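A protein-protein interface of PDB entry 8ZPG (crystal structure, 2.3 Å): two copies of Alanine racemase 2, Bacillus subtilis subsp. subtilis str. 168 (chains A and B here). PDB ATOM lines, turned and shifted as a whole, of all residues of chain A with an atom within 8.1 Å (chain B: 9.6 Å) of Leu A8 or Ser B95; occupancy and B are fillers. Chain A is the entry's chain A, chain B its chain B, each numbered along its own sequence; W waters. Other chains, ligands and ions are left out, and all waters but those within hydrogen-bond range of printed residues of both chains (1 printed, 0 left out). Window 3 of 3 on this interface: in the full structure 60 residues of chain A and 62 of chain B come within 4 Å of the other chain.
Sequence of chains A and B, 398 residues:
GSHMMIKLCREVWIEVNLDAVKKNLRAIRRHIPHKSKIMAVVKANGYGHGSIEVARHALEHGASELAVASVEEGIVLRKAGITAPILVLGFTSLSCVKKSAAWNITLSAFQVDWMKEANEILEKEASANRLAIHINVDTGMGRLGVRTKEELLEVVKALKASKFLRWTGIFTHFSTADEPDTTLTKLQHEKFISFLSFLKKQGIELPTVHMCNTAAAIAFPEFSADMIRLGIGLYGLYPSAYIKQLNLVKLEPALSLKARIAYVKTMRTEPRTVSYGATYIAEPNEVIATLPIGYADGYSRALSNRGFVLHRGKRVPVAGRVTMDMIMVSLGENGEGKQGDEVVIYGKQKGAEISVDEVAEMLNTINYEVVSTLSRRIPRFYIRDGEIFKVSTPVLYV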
ATOM      1  N   MET A   5       0.581 -28.782  35.925  1.00  0.00           N
ATOM      2  CA  MET A   5       0.017 -27.634  35.232  1.00  0.00           C
ATOM      3  C   MET A   5      -0.526 -28.025  33.843  1.00  0.00           C
ATOM      4  O   MET A   5      -1.225 -29.034  33.697  1.00  0.00           O
ATOM      5  CB  MET A   5       1.071 -26.520  35.118  1.00  0.00           C
ATOM      6  CG  MET A   5       0.503 -25.082  35.130  1.00  0.00           C
ATOM      7  SD  MET A   5      -0.989 -24.782  36.142  1.00  0.00           S
ATOM      8  CE  MET A   5      -0.668 -25.679  37.677  1.00  0.00           C
ATOM      9  N   ILE A   6      -0.189 -27.220  32.832  1.00  0.00           N
ATOM     10  CA  ILE A   6      -0.778 -27.285  31.494  1.00  0.00           C
ATOM     11  C   ILE A   6       0.326 -27.649  30.501  1.00  0.00           C
ATOM     12  O   ILE A   6       1.361 -26.976  30.456  1.00  0.00           O
ATOM     13  CB  ILE A   6      -1.437 -25.937  31.133  1.00  0.00           C
ATOM     14  CG1 ILE A   6      -2.733 -25.733  31.929  1.00  0.00           C
ATOM     15  CG2 ILE A   6      -1.692 -25.827  29.644  1.00  0.00           C
ATOM     16  CD1 ILE A   6      -2.904 -24.337  32.486  1.00  0.00           C
ATOM     17  N   LYS A   7       0.103 -28.707  29.701  1.00  0.00           N
ATOM     18  CA  LYS A   7       1.137 -29.318  28.850  1.00  0.00           C
ATOM     19  C   LYS A   7       0.723 -29.271  27.378  1.00  0.00           C
ATOM     20  O   LYS A   7      -0.134 -30.047  26.949  1.00  0.00           O
ATOM     21  CB  LYS A   7       1.403 -30.767  29.272  1.00  0.00           C
ATOM     22  CG  LYS A   7       2.153 -30.928  30.595  1.00  0.00           C
ATOM     23  CD  LYS A   7       1.517 -31.991  31.492  1.00  0.00           C
ATOM     24  CE  LYS A   7       2.470 -32.447  32.608  1.00  0.00           C
ATOM     25  NZ  LYS A   7       1.898 -33.547  33.461  1.00  0.00           N
ATOM     26  N   LEU A   8       1.366 -28.406  26.594  1.00  0.00           N
ATOM     27  CA  LEU A   8       1.005 -28.197  25.200  1.00  0.00           C
ATOM     28  C   LEU A   8       2.238 -28.221  24.308  1.00  0.00           C
ATOM     29  O   LEU A   8       3.370 -28.041  24.764  1.00  0.00           O
ATOM     30  CB  LEU A   8       0.282 -26.864  25.027  1.00  0.00           C
ATOM     31  CG  LEU A   8      -0.939 -26.666  25.918  1.00  0.00           C
ATOM     32  CD1 LEU A   8      -1.228 -25.173  26.116  1.00  0.00           C
ATOM     33  CD2 LEU A   8      -2.136 -27.390  25.301  1.00  0.00           C
ATOM     34  N   CYS A   9       2.006 -28.428  23.010  1.00  0.00           N
ATOM     35  CA  CYS A   9       3.090 -28.331  22.037  1.00  0.00           C
ATOM     36  C   CYS A   9       3.329 -26.874  21.646  1.00  0.00           C
ATOM     37  O   CYS A   9       4.459 -26.376  21.740  1.00  0.00           O
ATOM     38  CB  CYS A   9       2.779 -29.193  20.802  1.00  0.00           C
ATOM     39  SG  CYS A   9       2.526 -31.010  21.075  1.00  0.00           S
ATOM     40  N   ARG A  10       2.263 -26.184  21.210  1.00  0.00           N
ATOM     41  CA  ARG A  10       2.220 -24.727  21.061  1.00  0.00           C
ATOM     42  C   ARG A  10       1.534 -24.127  22.295  1.00  0.00           C
ATOM     43  O   ARG A  10       0.394 -24.481  22.614  1.00  0.00           O
ATOM     44  CB  ARG A  10       1.476 -24.342  19.778  1.00  0.00           C
ATOM     45  CG  ARG A  10       1.411 -22.857  19.478  1.00  0.00           C
ATOM     46  CD  ARG A  10       0.171 -22.549  18.634  1.00  0.00           C
ATOM     47  NE  ARG A  10       0.198 -21.219  18.026  1.00  0.00           N
ATOM     48  CZ  ARG A  10      -0.874 -20.519  17.679  1.00  0.00           C
ATOM     49  NH1 ARG A  10      -2.104 -20.959  17.910  1.00  0.00           N
ATOM     50  NH2 ARG A  10      -0.709 -19.354  17.060  1.00  0.00           N
ATOM     51  N   GLU A  11       2.210 -23.209  22.977  1.00  0.00           N
ATOM     52  CA  GLU A  11       1.823 -22.853  24.347  1.00  0.00           C
ATOM     53  C   GLU A  11       0.978 -21.575  24.405  1.00  0.00           C
ATOM     54  O   GLU A  11       1.438 -20.511  24.835  1.00  0.00           O
ATOM     55  CB  GLU A  11       3.074 -22.734  25.211  1.00  0.00           C
ATOM     56  CG  GLU A  11       3.813 -24.056  25.316  1.00  0.00           C
ATOM     57  CD  GLU A  11       5.195 -23.927  25.927  1.00  0.00           C
ATOM     58  OE1 GLU A  11       6.065 -23.349  25.259  1.00  0.00           O
ATOM     59  OE2 GLU A  11       5.417 -24.414  27.062  1.00  0.00           O
ATOM     60  N   VAL A  12      -0.304 -21.717  24.030  1.00  0.00           N
ATOM     61  CA  VAL A  12      -1.306 -20.655  24.142  1.00  0.00           C
ATOM     62  C   VAL A  12      -2.661 -21.286  24.497  1.00  0.00           C
ATOM     63  O   VAL A  12      -3.021 -22.338  23.955  1.00  0.00           O
ATOM     64  CB  VAL A  12      -1.388 -19.805  22.839  1.00  0.00           C
ATOM     65  CG1 VAL A  12      -1.515 -20.669  21.578  1.00  0.00           C
ATOM     66  CG2 VAL A  12      -2.545 -18.826  22.895  1.00  0.00           C
ATOM     67  N   TRP A  13      -3.418 -20.647  25.407  1.00  0.00           N
ATOM     68  CA  TRP A  13      -4.651 -21.256  25.922  1.00  0.00           C
ATOM     69  C   TRP A  13      -5.583 -20.212  26.552  1.00  0.00           C
ATOM     70  O   TRP A  13      -5.180 -19.078  26.850  1.00  0.00           O
ATOM     71  CB  TRP A  13      -4.326 -22.387  26.929  1.00  0.00           C
ATOM     72  CG  TRP A  13      -3.772 -21.950  28.272  1.00  0.00           C
ATOM     73  CD1 TRP A  13      -4.483 -21.738  29.420  1.00  0.00           C
ATOM     74  CD2 TRP A  13      -2.399 -21.675  28.597  1.00  0.00           C
ATOM     75  NE1 TRP A  13      -3.641 -21.343  30.434  1.00  0.00           N
ATOM     76  CE2 TRP A  13      -2.359 -21.292  29.952  1.00  0.00           C
ATOM     77  CE3 TRP A  13      -1.207 -21.689  27.868  1.00  0.00           C
ATOM     78  CZ2 TRP A  13      -1.168 -20.950  30.596  1.00  0.00           C
ATOM     79  CZ3 TRP A  13      -0.027 -21.338  28.506  1.00  0.00           C
ATOM     80  CH2 TRP A  13      -0.015 -20.988  29.860  1.00  0.00           C
ATOM     81  N   ILE A  14      -6.852 -20.619  26.736  1.00  0.00           N
ATOM     82  CA  ILE A  14      -7.902 -19.821  27.390  1.00  0.00           C
ATOM     83  C   ILE A  14      -8.348 -20.527  28.677  1.00  0.00           C
ATOM     84  O   ILE A  14      -8.354 -21.762  28.758  1.00  0.00           O
ATOM     85  CB  ILE A  14      -9.114 -19.585  26.444  1.00  0.00           C
ATOM     86  CG1 ILE A  14      -8.857 -18.451  25.449  1.00  0.00           C
ATOM     87  CG2 ILE A  14     -10.407 -19.279  27.193  1.00  0.00           C
ATOM     88  CD1 ILE A  14      -9.728 -18.560  24.160  1.00  0.00           C
ATOM     89  N   LYS A 258      -3.764 -16.494  27.766  1.00  0.00           N
ATOM     90  CA  LYS A 258      -2.367 -16.581  28.209  1.00  0.00           C
ATOM     91  C   LYS A 258      -1.475 -17.301  27.194  1.00  0.00           C
ATOM     92  O   LYS A 258      -1.960 -17.998  26.300  1.00  0.00           O
ATOM     93  CB  LYS A 258      -2.239 -17.324  29.555  1.00  0.00           C
ATOM     94  CG  LYS A 258      -3.337 -17.026  30.550  1.00  0.00           C
ATOM     95  CD  LYS A 258      -3.036 -17.719  31.877  1.00  0.00           C
ATOM     96  CE  LYS A 258      -3.705 -17.019  33.054  1.00  0.00           C
ATOM     97  NZ  LYS A 258      -3.593 -17.804  34.335  1.00  0.00           N
ATOM     98  N   ALA A 259      -0.149 -17.141  27.365  1.00  0.00           N
ATOM     99  CA  ALA A 259       0.868 -17.891  26.618  1.00  0.00           C
ATOM    100  C   ALA A 259       2.151 -17.996  27.446  1.00  0.00           C
ATOM    101  O   ALA A 259       2.242 -17.480  28.563  1.00  0.00           O
ATOM    102  CB  ALA A 259       1.179 -17.243  25.260  1.00  0.00           C
ATOM    103  N   ARG A 260       3.149 -18.685  26.892  1.00  0.00           N
ATOM    104  CA  ARG A 260       4.502 -18.731  27.445  1.00  0.00           C
ATOM    105  C   ARG A 260       5.496 -18.250  26.399  1.00  0.00           C
ATOM    106  O   ARG A 260       5.352 -18.554  25.209  1.00  0.00           O
ATOM    107  CB  ARG A 260       4.914 -20.145  27.886  1.00  0.00           C
ATOM    108  CG  ARG A 260       4.017 -20.766  28.937  1.00  0.00           C
ATOM    109  CD  ARG A 260       4.768 -21.813  29.694  1.00  0.00           C
ATOM    110  NE  ARG A 260       4.103 -23.106  29.656  1.00  0.00           N
ATOM    111  CZ  ARG A 260       3.184 -23.492  30.530  1.00  0.00           C
ATOM    112  NH1 ARG A 260       2.810 -22.702  31.527  1.00  0.00           N
ATOM    113  NH2 ARG A 260       2.620 -24.693  30.397  1.00  0.00           N
ATOM    114  N   ILE A 378      -7.621 -22.560  19.577  1.00  0.00           N
ATOM    115  CA  ILE A 378      -7.084 -22.313  20.918  1.00  0.00           C
ATOM    116  C   ILE A 378      -7.817 -23.224  21.890  1.00  0.00           C
ATOM    117  O   ILE A 378      -9.059 -23.151  21.978  1.00  0.00           O
ATOM    118  CB  ILE A 378      -7.246 -20.853  21.360  1.00  0.00           C
ATOM    119  CG1 ILE A 378      -6.580 -19.845  20.420  1.00  0.00           C
ATOM    120  CG2 ILE A 378      -6.712 -20.672  22.813  1.00  0.00           C
ATOM    121  CD1 ILE A 378      -6.951 -18.353  20.813  1.00  0.00           C
ATOM    122  N   PRO A 379      -7.108 -24.046  22.672  1.00  0.00           N
ATOM    123  CA  PRO A 379      -7.770 -24.920  23.656  1.00  0.00           C
ATOM    124  C   PRO A 379      -8.334 -24.153  24.859  1.00  0.00           C
ATOM    125  O   PRO A 379      -7.732 -23.184  25.332  1.00  0.00           O
ATOM    126  CB  PRO A 379      -6.637 -25.855  24.083  1.00  0.00           C
ATOM    127  CG  PRO A 379      -5.397 -24.997  23.947  1.00  0.00           C
ATOM    128  CD  PRO A 379      -5.641 -24.184  22.708  1.00  0.00           C
ATOM    129  N   ARG A 380      -9.489 -24.617  25.360  1.00  0.00           N
ATOM    130  CA  ARG A 380     -10.215 -23.998  26.473  1.00  0.00           C
ATOM    131  C   ARG A 380     -10.191 -24.893  27.719  1.00  0.00           C
ATOM    132  O   ARG A 380     -10.529 -26.078  27.639  1.00  0.00           O
ATOM    133  CB  ARG A 380     -11.676 -23.730  26.081  1.00  0.00           C
ATOM    134  CG  ARG A 380     -11.930 -22.441  25.327  1.00  0.00           C
ATOM    135  CD  ARG A 380     -12.572 -22.690  23.975  1.00  0.00           C
ATOM    136  NE  ARG A 380     -12.937 -21.460  23.297  1.00  0.00           N
ATOM    137  CZ  ARG A 380     -12.300 -20.954  22.249  1.00  0.00           C
ATOM    138  NH1 ARG A 380     -11.201 -21.521  21.768  1.00  0.00           N
ATOM    139  NH2 ARG A 380     -12.779 -19.856  21.665  1.00  0.00           N
ATOM    140  N   PHE A 381      -9.854 -24.310  28.876  1.00  0.00           N
ATOM    141  CA  PHE A 381      -9.832 -25.002  30.169  1.00  0.00           C
ATOM    142  C   PHE A 381     -10.841 -24.386  31.145  1.00  0.00           C
ATOM    143  O   PHE A 381     -11.008 -23.166  31.191  1.00  0.00           O
ATOM    144  CB  PHE A 381      -8.411 -24.973  30.776  1.00  0.00           C
ATOM    145  CG  PHE A 381      -7.361 -25.735  29.961  1.00  0.00           C
ATOM    146  CD1 PHE A 381      -6.854 -25.211  28.779  1.00  0.00           C
ATOM    147  CD2 PHE A 381      -6.868 -26.958  30.397  1.00  0.00           C
ATOM    148  CE1 PHE A 381      -5.896 -25.894  28.045  1.00  0.00           C
ATOM    149  CE2 PHE A 381      -5.892 -27.650  29.660  1.00  0.00           C
ATOM    150  CZ  PHE A 381      -5.412 -27.109  28.484  1.00  0.00           C
ATOM    151  N   SER B  70       2.241 -25.940  13.924  1.00  0.00           N
ATOM    152  CA  SER B  70       2.317 -26.595  15.220  1.00  0.00           C
ATOM    153  C   SER B  70       2.076 -28.087  15.055  1.00  0.00           C
ATOM    154  O   SER B  70       1.427 -28.526  14.101  1.00  0.00           O
ATOM    155  CB  SER B  70       1.273 -26.016  16.172  1.00  0.00           C
ATOM    156  OG  SER B  70      -0.016 -26.466  15.789  1.00  0.00           O
ATOM    157  N   VAL B  71       2.537 -28.852  16.048  1.00  0.00           N
ATOM    158  CA  VAL B  71       2.436 -30.308  15.985  1.00  0.00           C
ATOM    159  C   VAL B  71       0.984 -30.733  15.866  1.00  0.00           C
ATOM    160  O   VAL B  71       0.677 -31.755  15.240  1.00  0.00           O
ATOM    161  CB  VAL B  71       3.116 -30.943  17.220  1.00  0.00           C
ATOM    162  CG1 VAL B  71       2.658 -32.398  17.423  1.00  0.00           C
ATOM    163  CG2 VAL B  71       4.623 -30.862  17.109  1.00  0.00           C
ATOM    164  N   GLU B  72       0.062 -29.961  16.455  1.00  0.00           N
ATOM    165  CA  GLU B  72      -1.352 -30.335  16.416  1.00  0.00           C
ATOM    166  C   GLU B  72      -1.954 -30.175  15.016  1.00  0.00           C
ATOM    167  O   GLU B  72      -2.826 -30.961  14.623  1.00  0.00           O
ATOM    168  CB  GLU B  72      -2.138 -29.515  17.443  1.00  0.00           C
ATOM    169  CG  GLU B  72      -1.670 -29.698  18.891  1.00  0.00           C
ATOM    170  CD  GLU B  72      -0.559 -28.714  19.274  1.00  0.00           C
ATOM    171  OE1 GLU B  72       0.251 -28.373  18.389  1.00  0.00           O
ATOM    172  OE2 GLU B  72      -0.491 -28.282  20.454  1.00  0.00           O
ATOM    173  N   PHE B  91       7.957 -22.813  17.330  1.00  0.00           N
ATOM    174  CA  PHE B  91       8.659 -23.443  18.445  1.00  0.00           C
ATOM    175  C   PHE B  91       7.827 -24.552  19.090  1.00  0.00           C
ATOM    176  O   PHE B  91       6.673 -24.341  19.470  1.00  0.00           O
ATOM    177  CB  PHE B  91       9.024 -22.400  19.497  1.00  0.00           C
ATOM    178  CG  PHE B  91       9.763 -22.971  20.673  1.00  0.00           C
ATOM    179  CD1 PHE B  91      11.108 -23.278  20.570  1.00  0.00           C
ATOM    180  CD2 PHE B  91       9.111 -23.187  21.889  1.00  0.00           C
ATOM    181  CE1 PHE B  91      11.803 -23.799  21.654  1.00  0.00           C
ATOM    182  CE2 PHE B  91       9.790 -23.702  22.986  1.00  0.00           C
ATOM    183  CZ  PHE B  91      11.143 -24.014  22.873  1.00  0.00           C
ATOM    184  N   THR B  92       8.433 -25.720  19.265  1.00  0.00           N
ATOM    185  CA  THR B  92       7.784 -26.839  19.934  1.00  0.00           C
ATOM    186  C   THR B  92       8.459 -27.089  21.274  1.00  0.00           C
ATOM    187  O   THR B  92       9.692 -27.176  21.347  1.00  0.00           O
ATOM    188  CB  THR B  92       7.836 -28.101  19.074  1.00  0.00           C
ATOM    189  OG1 THR B  92       7.253 -27.831  17.788  1.00  0.00           O
ATOM    190  CG2 THR B  92       7.112 -29.256  19.759  1.00  0.00           C
ATOM    191  N   SER B  93       7.645 -27.217  22.321  1.00  0.00           N
ATOM    192  CA  SER B  93       8.171 -27.477  23.649  1.00  0.00           C
ATOM    193  C   SER B  93       8.683 -28.912  23.784  1.00  0.00           C
ATOM    194  O   SER B  93       8.174 -29.849  23.164  1.00  0.00           O
ATOM    195  CB  SER B  93       7.099 -27.194  24.708  1.00  0.00           C
ATOM    196  OG  SER B  93       6.428 -28.370  25.085  1.00  0.00           O
ATOM    197  N   LEU B  94       9.704 -29.070  24.628  1.00  0.00           N
ATOM    198  CA  LEU B  94      10.289 -30.374  24.898  1.00  0.00           C
ATOM    199  C   LEU B  94       9.255 -31.397  25.366  1.00  0.00           C
ATOM    200  O   LEU B  94       9.477 -32.604  25.217  1.00  0.00           O
ATOM    201  CB  LEU B  94      11.417 -30.226  25.930  1.00  0.00           C
ATOM    202  CG  LEU B  94      12.765 -29.656  25.432  1.00  0.00           C
ATOM    203  CD1 LEU B  94      13.682 -29.360  26.604  1.00  0.00           C
ATOM    204  CD2 LEU B  94      13.484 -30.555  24.425  1.00  0.00           C
ATOM    205  N   SER B  95       8.118 -30.957  25.909  1.00  0.00           N
ATOM    206  CA  SER B  95       7.131 -31.936  26.350  1.00  0.00           C
ATOM    207  C   SER B  95       6.492 -32.690  25.189  1.00  0.00           C
ATOM    208  O   SER B  95       5.775 -33.666  25.432  1.00  0.00           O
ATOM    209  CB  SER B  95       6.052 -31.261  27.206  1.00  0.00           C
ATOM    210  OG  SER B  95       5.205 -30.421  26.441  1.00  0.00           O
ATOM    211  N   CYS B  96       6.727 -32.277  23.944  1.00  0.00           N
ATOM    212  CA  CYS B  96       6.153 -32.968  22.796  1.00  0.00           C
ATOM    213  C   CYS B  96       7.211 -33.684  21.936  1.00  0.00           C
ATOM    214  O   CYS B  96       6.913 -34.061  20.788  1.00  0.00           O
ATOM    215  CB  CYS B  96       5.327 -31.988  21.948  1.00  0.00           C
ATOM    216  SG  CYS B  96       3.694 -31.591  22.652  1.00  0.00           S
ATOM    217  N   VAL B  97       8.424 -33.910  22.468  1.00  0.00           N
ATOM    218  CA  VAL B  97       9.460 -34.600  21.685  1.00  0.00           C
ATOM    219  C   VAL B  97       9.054 -36.052  21.401  1.00  0.00           C
ATOM    220  O   VAL B  97       9.104 -36.505  20.252  1.00  0.00           O
ATOM    221  CB  VAL B  97      10.839 -34.517  22.377  1.00  0.00           C
ATOM    222  CG1 VAL B  97      11.804 -35.471  21.744  1.00  0.00           C
ATOM    223  CG2 VAL B  97      11.442 -33.116  22.256  1.00  0.00           C
ATOM    224  N   LYS B  98       8.638 -36.803  22.431  1.00  0.00           N
ATOM    225  CA  LYS B  98       8.255 -38.205  22.218  1.00  0.00           C
ATOM    226  C   LYS B  98       7.078 -38.345  21.235  1.00  0.00           C
ATOM    227  O   LYS B  98       7.047 -39.265  20.404  1.00  0.00           O
ATOM    228  CB  LYS B  98       7.920 -38.858  23.564  1.00  0.00           C
ATOM    229  CG  LYS B  98       7.147 -40.164  23.425  1.00  0.00           C
ATOM    230  CD  LYS B  98       7.684 -41.240  24.349  1.00  0.00           C
ATOM    231  CE  LYS B  98       6.757 -42.464  24.389  1.00  0.00           C
ATOM    232  NZ  LYS B  98       7.294 -43.652  23.656  1.00  0.00           N
ATOM    233  N   LYS B  99       6.112 -37.428  21.303  1.00  0.00           N
ATOM    234  CA  LYS B  99       4.923 -37.485  20.457  1.00  0.00           C
ATOM    235  C   LYS B  99       5.246 -37.180  18.996  1.00  0.00           C
ATOM    236  O   LYS B  99       4.665 -37.783  18.083  1.00  0.00           O
ATOM    237  CB  LYS B  99       3.885 -36.497  20.999  1.00  0.00           C
ATOM    238  CG  LYS B  99       2.643 -36.402  20.180  1.00  0.00           C
ATOM    239  CD  LYS B  99       1.436 -36.069  21.038  1.00  0.00           C
ATOM    240  CE  LYS B  99       1.461 -34.628  21.492  1.00  0.00           C
ATOM    241  NZ  LYS B  99       0.115 -34.232  22.024  1.00  0.00           N
ATOM    242  N   SER B 100       6.138 -36.215  18.756  1.00  0.00           N
ATOM    243  CA  SER B 100       6.569 -35.888  17.398  1.00  0.00           C
ATOM    244  C   SER B 100       7.340 -37.033  16.766  1.00  0.00           C
ATOM    245  O   SER B 100       7.257 -37.247  15.552  1.00  0.00           O
ATOM    246  CB  SER B 100       7.443 -34.632  17.411  1.00  0.00           C
ATOM    247  OG  SER B 100       6.760 -33.527  18.000  1.00  0.00           O
ATOM    248  N   ALA B 101       8.104 -37.766  17.566  1.00  0.00           N
ATOM    249  CA  ALA B 101       8.842 -38.895  17.029  1.00  0.00           C
ATOM    250  C   ALA B 101       7.905 -40.016  16.602  1.00  0.00           C
ATOM    251  O   ALA B 101       8.194 -40.715  15.635  1.00  0.00           O
ATOM    252  CB  ALA B 101       9.866 -39.376  18.062  1.00  0.00           C
ATOM    253  N   LEU B 107      10.716 -30.897  13.073  1.00  0.00           N
ATOM    254  CA  LEU B 107      10.656 -29.717  13.928  1.00  0.00           C
ATOM    255  C   LEU B 107      11.826 -28.777  13.656  1.00  0.00           C
ATOM    256  O   LEU B 107      12.918 -29.215  13.278  1.00  0.00           O
ATOM    257  CB  LEU B 107      10.660 -30.128  15.417  1.00  0.00           C
ATOM    258  CG  LEU B 107       9.743 -31.285  15.839  1.00  0.00           C
ATOM    259  CD1 LEU B 107      10.211 -31.928  17.131  1.00  0.00           C
ATOM    260  CD2 LEU B 107       8.291 -30.820  15.984  1.00  0.00           C
ATOM    261  N   TRP B 114      18.611 -27.344  23.873  1.00  0.00           N
ATOM    262  CA  TRP B 114      17.403 -28.013  23.405  1.00  0.00           C
ATOM    263  C   TRP B 114      17.753 -29.291  22.630  1.00  0.00           C
ATOM    264  O   TRP B 114      17.204 -30.371  22.901  1.00  0.00           O
ATOM    265  CB  TRP B 114      16.597 -27.010  22.554  1.00  0.00           C
ATOM    266  CG  TRP B 114      15.179 -27.430  22.204  1.00  0.00           C
ATOM    267  CD1 TRP B 114      14.016 -27.043  22.827  1.00  0.00           C
ATOM    268  CD2 TRP B 114      14.785 -28.315  21.140  1.00  0.00           C
ATOM    269  NE1 TRP B 114      12.930 -27.633  22.211  1.00  0.00           N
ATOM    270  CE2 TRP B 114      13.380 -28.425  21.183  1.00  0.00           C
ATOM    271  CE3 TRP B 114      15.488 -29.032  20.167  1.00  0.00           C
ATOM    272  CZ2 TRP B 114      12.674 -29.222  20.291  1.00  0.00           C
ATOM    273  CZ3 TRP B 114      14.783 -29.822  19.292  1.00  0.00           C
ATOM    274  CH2 TRP B 114      13.393 -29.905  19.351  1.00  0.00           C
ATOM    275  N   GLU B 117      18.903 -31.947  25.320  1.00  0.00           N
ATOM    276  CA  GLU B 117      17.812 -32.555  26.084  1.00  0.00           C
ATOM    277  C   GLU B 117      16.838 -33.328  25.199  1.00  0.00           C
ATOM    278  O   GLU B 117      16.308 -34.357  25.623  1.00  0.00           O
ATOM    279  CB  GLU B 117      17.075 -31.479  26.884  1.00  0.00           C
ATOM    280  CG  GLU B 117      17.989 -30.704  27.834  1.00  0.00           C
ATOM    281  CD  GLU B 117      18.147 -31.393  29.196  1.00  0.00           C
ATOM    282  OE1 GLU B 117      17.143 -31.946  29.697  1.00  0.00           O
ATOM    283  OE2 GLU B 117      19.267 -31.387  29.767  1.00  0.00           O
ATOM    284  N   ALA B 118      16.576 -32.863  23.974  1.00  0.00           N
ATOM    285  CA  ALA B 118      15.741 -33.659  23.076  1.00  0.00           C
ATOM    286  C   ALA B 118      16.337 -35.046  22.850  1.00  0.00           C
ATOM    287  O   ALA B 118      15.620 -36.056  22.896  1.00  0.00           O
ATOM    288  CB  ALA B 118      15.547 -32.938  21.739  1.00  0.00           C
ATOM    289  N   ILE B 121      15.865 -37.388  25.863  1.00  0.00           N
ATOM    290  CA  ILE B 121      14.510 -37.915  26.053  1.00  0.00           C
ATOM    291  C   ILE B 121      14.325 -39.217  25.271  1.00  0.00           C
ATOM    292  O   ILE B 121      13.855 -40.223  25.812  1.00  0.00           O
ATOM    293  CB  ILE B 121      13.455 -36.855  25.674  1.00  0.00           C
ATOM    294  CG1 ILE B 121      13.349 -35.776  26.763  1.00  0.00           C
ATOM    295  CG2 ILE B 121      12.084 -37.501  25.461  1.00  0.00           C
ATOM    296  CD1 ILE B 121      12.658 -34.480  26.302  1.00  0.00           C
HETATM  297  O   HOH W   1       4.978 -22.914  21.892  1.00  0.00           O
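Of the 19 printed residues of chain B, 9 touch a printed residue of chain A.
Leu A8 touches just these residues of chain B: Ser B93 (3.1 Å) and Ser B95 (3.4 Å).
Cys A9 touches just these residues of chain B: Val B71, Glu B72, Phe B91, Thr B92, Ser B93, Cys B96 and Lys B99.
Of chain B, only Ser B93 (3.97 Å) comes within 4 Å of Glu A11.
Ile A14 touches none of the printed residues of chain B.
Ala A259 touches none of the printed residues of chain B.
Printed residues of chain A within 4 Å of Glu B72: Cys A9 (3.4 Å) and Arg A10 (3.5 Å).
Of the printed residues of chain A, Thr B92 touches Cys A9 (3.8 Å).
Ser B95 touches just one residue of chain A: Leu A8 (3.4 Å).
The nearest printed residue of chain A that does not touch Phe B91 is Glu A11 (4.4 Å).
Among the printed residues, pairs that only touch across the chains: Cys A9 with Val B71 (3.9 Å), Cys A9 with Glu B72 (3.4 Å), Cys A9 with Phe B91 (3.8 Å), Cys A9 with Thr B92 (3.8 Å), Cys A9 with Lys B99 (3.8 Å), Arg A10 with Ser B70 (3.98 Å), Arg A10 with Glu B72 (3.5 Å) and Glu A11 with Ser B93 (3.97 Å).
The backbone carbonyl oxygen (O) of Leu A8 is in hydrogen-bond range of the side-chain hydroxyl (OG) of Ser B95, 3.4 Å away.
The backbone carbonyl oxygen of Leu A8 lies within hydrogen-bond range of the side-chain hydroxyl of Ser B93 (3.1 Å).
The side-chain sulfur of Cys A9 is disulfide-bonded to the side-chain sulfur of Cys B96 (2.0 Å).
N of Ser B93 is in hydrogen-bond range of O of Cys A9 (3.3 Å).
The side-chain hydroxyl (OG) of Ser B100 is in hydrogen-bond range of the backbone carbonyl oxygen (O) of Cys B96 (2.8 Å).
The backbone carbonyl oxygen (O) of Thr B92 lies within hydrogen-bond range of the indole nitrogen (NE1) of Trp B114 (3.4 Å).
NE of Arg A260 is in salt-bridge range of OE2 of Glu A11 (3.2 Å).
The side-chain hydroxyl (OG) of Ser B95 lies within hydrogen-bond range of the side-chain hydroxyl (OG) of Ser B93.
The side-chain hydroxyl (OG) of Ser B70 sits at hydrogen-bond distance from the side-chain carboxylate (OE1) of Glu B72, 3.2 Å away.
Water W1 lies within hydrogen-bond range of N of Glu A11 and O of Phe B91.
No position is printed for both chains.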
